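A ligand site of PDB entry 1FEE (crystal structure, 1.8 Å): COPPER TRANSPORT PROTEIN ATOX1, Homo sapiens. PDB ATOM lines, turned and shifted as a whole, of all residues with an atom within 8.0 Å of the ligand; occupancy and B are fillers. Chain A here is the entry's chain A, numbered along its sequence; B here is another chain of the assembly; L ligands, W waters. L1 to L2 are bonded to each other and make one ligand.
OH of Tyr 31 sits at hydrogen-bond distance from OG of Ser 20, at 2.6 Å.
NH1 of Arg 21 is in hydrogen-bond range of O of Gly 59 of chain B (2.7 Å).
The side-chain amide nitrogen (ND2) of Asn 24 lies close to the backbone carbonyl oxygen (O) of Ser 20 (3.3 Å).
The side-chain carboxylate (OE2) of Glu 17 lies within salt-bridge range of the guanidinium group (NH2) of Arg 21 (3.7 Å).
The side-chain hydroxyl (OH) of Tyr 31 lies within hydrogen-bond range of the side-chain amide nitrogen (ND2) of Asn 24 (2.6 Å).
Water W3 bridges O1 of LG2 L2 (2.4 Å) and OG of Ser 20 (2.7 Å).
Water W2 bridges the backbone carbonyl oxygen of Arg 21 (2.8 Å) and an oxygen (O4) of LG2 L2 (2.9 Å).
An oxygen (O1) of LG2 L2 sits at hydrogen-bond distance from the backbone carbonyl oxygen (O) of Glu 17 (3.1 Å).
O3 of LG2 L2 lies within hydrogen-bond range of OG of Ser 20, 3.3 Å away.
OD1 of Asn 24 is in hydrogen-bond range of O3 of LG2 L2, 2.5 Å away.
The guanidinium group (NH2) of Arg 21 sits at hydrogen-bond distance from an oxygen (O5) of LG2 L2 (3.0 Å).
Of the 18 residues printed, 4 come within 4 Å of the ligand.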
ATOM      1  N   GLY A  13     -13.683  -7.945  17.620  1.00  0.00           N
ATOM      2  CA  GLY A  13     -14.904  -8.204  16.886  1.00  0.00           C
ATOM      3  C   GLY A  13     -14.671  -8.248  15.380  1.00  0.00           C
ATOM      4  O   GLY A  13     -15.359  -8.961  14.655  1.00  0.00           O
ATOM      5  N   GLY A  14     -13.704  -7.467  14.917  1.00  0.00           N
ATOM      6  CA  GLY A  14     -13.385  -7.441  13.505  1.00  0.00           C
ATOM      7  C   GLY A  14     -12.830  -8.785  13.065  1.00  0.00           C
ATOM      8  O   GLY A  14     -13.059  -9.217  11.935  1.00  0.00           O
ATOM      9  N   CYS A  15     -12.106  -9.442  13.964  1.00  0.00           N
ATOM     10  CA  CYS A  15     -11.534 -10.765  13.666  1.00  0.00           C
ATOM     11  C   CYS A  15     -12.677 -11.774  13.450  1.00  0.00           C
ATOM     12  O   CYS A  15     -12.630 -12.591  12.544  1.00  0.00           O
ATOM     13  CB  CYS A  15     -10.652 -11.247  14.830  1.00  0.00           C
ATOM     14  SG  CYS A  15      -8.962 -10.550  14.907  1.00  0.00           S
ATOM     15  N   ALA A  16     -13.690 -11.707  14.320  1.00  0.00           N
ATOM     16  CA  ALA A  16     -14.834 -12.603  14.222  1.00  0.00           C
ATOM     17  C   ALA A  16     -15.641 -12.307  12.959  1.00  0.00           C
ATOM     18  O   ALA A  16     -16.118 -13.226  12.281  1.00  0.00           O
ATOM     19  CB  ALA A  16     -15.719 -12.474  15.449  1.00  0.00           C
ATOM     20  N   GLU A  17     -15.811 -11.026  12.662  1.00  0.00           N
ATOM     21  CA  GLU A  17     -16.542 -10.616  11.472  1.00  0.00           C
ATOM     22  C   GLU A  17     -15.875 -11.188  10.217  1.00  0.00           C
ATOM     23  O   GLU A  17     -16.544 -11.631   9.282  1.00  0.00           O
ATOM     24  CB  GLU A  17     -16.591  -9.086  11.402  1.00  0.00           C
ATOM     25  CG  GLU A  17     -17.169  -8.529  10.117  1.00  0.00           C
ATOM     26  CD  GLU A  17     -17.044  -7.013  10.032  1.00  0.00           C
ATOM     27  OE1 GLU A  17     -15.919  -6.498  10.184  1.00  0.00           O
ATOM     28  OE2 GLU A  17     -18.067  -6.344   9.802  1.00  0.00           O
ATOM     29  N   ALA A  18     -14.540 -11.176  10.207  1.00  0.00           N
ATOM     30  CA  ALA A  18     -13.788 -11.685   9.062  1.00  0.00           C
ATOM     31  C   ALA A  18     -14.059 -13.173   8.864  1.00  0.00           C
ATOM     32  O   ALA A  18     -14.222 -13.634   7.731  1.00  0.00           O
ATOM     33  CB  ALA A  18     -12.296 -11.434   9.254  1.00  0.00           C
ATOM     34  N   VAL A  19     -14.088 -13.915   9.956  1.00  0.00           N
ATOM     35  CA  VAL A  19     -14.350 -15.354   9.907  1.00  0.00           C
ATOM     36  C   VAL A  19     -15.767 -15.588   9.365  1.00  0.00           C
ATOM     37  O   VAL A  19     -15.988 -16.462   8.531  1.00  0.00           O
ATOM     38  CB  VAL A  19     -14.211 -15.994  11.311  1.00  0.00           C
ATOM     39  CG1 VAL A  19     -14.665 -17.435  11.277  1.00  0.00           C
ATOM     40  CG2 VAL A  19     -12.761 -15.905  11.763  1.00  0.00           C
ATOM     41  N   SER A  20     -16.718 -14.793   9.854  1.00  0.00           N
ATOM     42  CA  SER A  20     -18.099 -14.910   9.411  1.00  0.00           C
ATOM     43  C   SER A  20     -18.233 -14.669   7.916  1.00  0.00           C
ATOM     44  O   SER A  20     -18.978 -15.363   7.215  1.00  0.00           O
ATOM     45  CB  SER A  20     -18.978 -13.903  10.167  1.00  0.00           C
ATOM     46  OG  SER A  20     -20.323 -13.948   9.723  1.00  0.00           O
ATOM     47  N   ARG A  21     -17.502 -13.671   7.414  1.00  0.00           N
ATOM     48  CA  ARG A  21     -17.543 -13.332   5.994  1.00  0.00           C
ATOM     49  C   ARG A  21     -17.043 -14.440   5.073  1.00  0.00           C
ATOM     50  O   ARG A  21     -17.677 -14.745   4.073  1.00  0.00           O
ATOM     51  CB  ARG A  21     -16.757 -12.038   5.751  1.00  0.00           C
ATOM     52  CG  ARG A  21     -16.776 -11.559   4.307  1.00  0.00           C
ATOM     53  CD  ARG A  21     -16.351 -10.096   4.223  1.00  0.00           C
ATOM     54  NE  ARG A  21     -17.311  -9.208   4.871  1.00  0.00           N
ATOM     55  CZ  ARG A  21     -17.023  -8.366   5.857  1.00  0.00           C
ATOM     56  NH1 ARG A  21     -15.789  -8.279   6.325  1.00  0.00           N
ATOM     57  NH2 ARG A  21     -17.974  -7.599   6.370  1.00  0.00           N
ATOM     58  N   VAL A  22     -15.905 -15.058   5.419  1.00  0.00           N
ATOM     59  CA  VAL A  22     -15.369 -16.112   4.565  1.00  0.00           C
ATOM     60  C   VAL A  22     -16.242 -17.376   4.610  1.00  0.00           C
ATOM     61  O   VAL A  22     -16.352 -18.086   3.618  1.00  0.00           O
ATOM     62  CB  VAL A  22     -13.901 -16.474   4.917  1.00  0.00           C
ATOM     63  CG1 VAL A  22     -13.020 -15.231   4.790  1.00  0.00           C
ATOM     64  CG2 VAL A  22     -13.799 -17.075   6.322  1.00  0.00           C
ATOM     65  N   LEU A  23     -16.865 -17.644   5.761  1.00  0.00           N
ATOM     66  CA  LEU A  23     -17.718 -18.816   5.861  1.00  0.00           C
ATOM     67  C   LEU A  23     -18.991 -18.592   5.043  1.00  0.00           C
ATOM     68  O   LEU A  23     -19.520 -19.527   4.440  1.00  0.00           O
ATOM     69  CB  LEU A  23     -18.069 -19.130   7.318  1.00  0.00           C
ATOM     70  CG  LEU A  23     -16.890 -19.629   8.169  1.00  0.00           C
ATOM     71  CD1 LEU A  23     -17.356 -19.923   9.586  1.00  0.00           C
ATOM     72  CD2 LEU A  23     -16.312 -20.902   7.533  1.00  0.00           C
ATOM     73  N   ASN A  24     -19.481 -17.358   5.025  1.00  0.00           N
ATOM     74  CA  ASN A  24     -20.674 -17.034   4.264  1.00  0.00           C
ATOM     75  C   ASN A  24     -20.379 -17.138   2.765  1.00  0.00           C
ATOM     76  O   ASN A  24     -21.239 -17.530   1.989  1.00  0.00           O
ATOM     77  CB  ASN A  24     -21.161 -15.613   4.574  1.00  0.00           C
ATOM     78  CG  ASN A  24     -21.882 -15.536   5.902  1.00  0.00           C
ATOM     79  OD1 ASN A  24     -22.372 -14.474   6.290  1.00  0.00           O
ATOM     80  ND2 ASN A  24     -21.973 -16.651   6.609  1.00  0.00           N
ATOM     81  N   LYS A  25     -19.165 -16.771   2.381  1.00  0.00           N
ATOM     82  CA  LYS A  25     -18.759 -16.837   0.979  1.00  0.00           C
ATOM     83  C   LYS A  25     -18.742 -18.301   0.542  1.00  0.00           C
ATOM     84  O   LYS A  25     -19.143 -18.630  -0.572  1.00  0.00           O
ATOM     85  CB  LYS A  25     -17.372 -16.216   0.798  1.00  0.00           C
ATOM     86  CG  LYS A  25     -16.945 -16.091  -0.661  1.00  0.00           C
ATOM     87  CD  LYS A  25     -15.604 -15.382  -0.782  1.00  0.00           C
ATOM     88  CE  LYS A  25     -15.193 -15.240  -2.245  1.00  0.00           C
ATOM     89  NZ  LYS A  25     -15.081 -16.561  -2.921  1.00  0.00           N
ATOM     90  N   TYR A  31     -23.167 -21.740  11.587  1.00  0.00           N
ATOM     91  CA  TYR A  31     -22.053 -21.627  12.520  1.00  0.00           C
ATOM     92  C   TYR A  31     -22.289 -20.646  13.658  1.00  0.00           C
ATOM     93  O   TYR A  31     -23.235 -19.857  13.641  1.00  0.00           O
ATOM     94  CB  TYR A  31     -20.793 -21.216  11.748  1.00  0.00           C
ATOM     95  CG  TYR A  31     -20.933 -19.878  11.038  1.00  0.00           C
ATOM     96  CD1 TYR A  31     -20.709 -18.682  11.715  1.00  0.00           C
ATOM     97  CD2 TYR A  31     -21.346 -19.814   9.707  1.00  0.00           C
ATOM     98  CE1 TYR A  31     -20.897 -17.451  11.086  1.00  0.00           C
ATOM     99  CE2 TYR A  31     -21.537 -18.584   9.064  1.00  0.00           C
ATOM    100  CZ  TYR A  31     -21.321 -17.401   9.767  1.00  0.00           C
ATOM    101  OH  TYR A  31     -21.512 -16.199   9.149  1.00  0.00           O
ATOM    102  N   ILE A  33     -19.795 -18.220  16.525  1.00  0.00           N
ATOM    103  CA  ILE A  33     -18.452 -17.803  16.884  1.00  0.00           C
ATOM    104  C   ILE A  33     -18.426 -17.309  18.317  1.00  0.00           C
ATOM    105  O   ILE A  33     -19.268 -16.512  18.727  1.00  0.00           O
ATOM    106  CB  ILE A  33     -17.966 -16.664  15.943  1.00  0.00           C
ATOM    107  CG1 ILE A  33     -17.963 -17.153  14.486  1.00  0.00           C
ATOM    108  CG2 ILE A  33     -16.566 -16.207  16.348  1.00  0.00           C
ATOM    109  CD1 ILE A  33     -17.698 -16.056  13.468  1.00  0.00           C
ATOM    110  N   GLY B  59     -10.919 -11.838   4.700  1.00  0.00           N
ATOM    111  CA  GLY B  59     -12.315 -11.690   5.089  1.00  0.00           C
ATOM    112  C   GLY B  59     -12.589 -10.272   5.563  1.00  0.00           C
ATOM    113  O   GLY B  59     -13.702  -9.959   6.009  1.00  0.00           O
ATOM    114  N   LYS B  60     -11.585  -9.409   5.476  1.00  0.00           N
ATOM    115  CA  LYS B  60     -11.732  -8.015   5.891  1.00  0.00           C
ATOM    116  C   LYS B  60     -12.155  -7.175   4.694  1.00  0.00           C
ATOM    117  O   LYS B  60     -11.959  -7.574   3.542  1.00  0.00           O
ATOM    118  CB  LYS B  60     -10.410  -7.483   6.441  1.00  0.00           C
ATOM    119  CG  LYS B  60      -9.878  -8.232   7.664  1.00  0.00           C
ATOM    120  CD  LYS B  60      -8.528  -7.663   8.070  1.00  0.00           C
ATOM    121  CE  LYS B  60      -7.961  -8.360   9.301  1.00  0.00           C
ATOM    122  NZ  LYS B  60      -7.734  -9.816   9.081  1.00  0.00           N
ATOM    123  N   THR B  61     -12.741  -6.008   4.955  1.00  0.00           N
ATOM    124  CA  THR B  61     -13.175  -5.127   3.878  1.00  0.00           C
ATOM    125  C   THR B  61     -11.942  -4.470   3.275  1.00  0.00           C
ATOM    126  O   THR B  61     -11.138  -3.864   3.994  1.00  0.00           O
ATOM    127  CB  THR B  61     -14.130  -4.033   4.406  1.00  0.00           C
ATOM    128  OG1 THR B  61     -15.311  -4.661   4.939  1.00  0.00           O
ATOM    129  CG2 THR B  61     -14.521  -3.078   3.295  1.00  0.00           C
HETATM  130  C1  LIG L   1     -21.577  -8.226   8.173  1.00  0.00           C
HETATM  131  C2  LIG L   1     -22.301  -7.954   9.525  1.00  0.00           C
HETATM  132  C3  LIG L   1     -23.812  -8.216   9.400  1.00  0.00           C
HETATM  133  C4  LIG L   1     -24.377  -7.330   8.340  1.00  0.00           C
HETATM  134  C5  LIG L   1     -23.703  -7.636   6.991  1.00  0.00           C
HETATM  135  C6  LIG L   1     -24.239  -6.744   5.907  1.00  0.00           C
HETATM  136  O1  LIG L   1     -21.684  -8.774  10.535  1.00  0.00           O
HETATM  137  O2  LIG L   1     -24.430  -7.922  10.652  1.00  0.00           O
HETATM  138  O3  LIG L   1     -25.820  -7.583   8.245  1.00  0.00           O
HETATM  139  O4  LIG L   1     -22.235  -7.406   7.132  1.00  0.00           O
HETATM  140  O5  LIG L   1     -24.672  -7.528   4.790  1.00  0.00           O
HETATM  141  C1  LG2 L   2     -19.235 -10.375   7.856  1.00  0.00           C
HETATM  142  C2  LG2 L   2     -20.535 -10.267   7.062  1.00  0.00           C
HETATM  143  C3  LG2 L   2     -21.070 -11.630   6.528  1.00  0.00           C
HETATM  144  C4  LG2 L   2     -21.700 -11.224   5.210  1.00  0.00           C
HETATM  145  C5  LG2 L   2     -20.617 -10.252   4.736  1.00  0.00           C
HETATM  146  C6  LG2 L   2     -20.950  -9.328   3.595  1.00  0.00           C
HETATM  147  O1  LG2 L   2     -19.517 -10.707   9.212  1.00  0.00           O
HETATM  148  O2  LG2 L   2     -21.633  -9.644   7.860  1.00  0.00           O
HETATM  149  O3  LG2 L   2     -22.005 -12.229   7.406  1.00  0.00           O
HETATM  150  O4  LG2 L   2     -21.819 -12.378   4.364  1.00  0.00           O
HETATM  151  O5  LG2 L   2     -20.290  -9.499   5.910  1.00  0.00           O
HETATM  152  O6  LG2 L   2     -19.827  -8.610   3.162  1.00  0.00           O
HETATM  153  O   HOH W   1     -24.218 -10.637   7.507  1.00  0.00           O
HETATM  154  O   HOH W   2     -19.552 -13.119   2.674  1.00  0.00           O
HETATM  155  O   HOH W   3     -21.644 -11.656   9.894  1.00  0.00           O
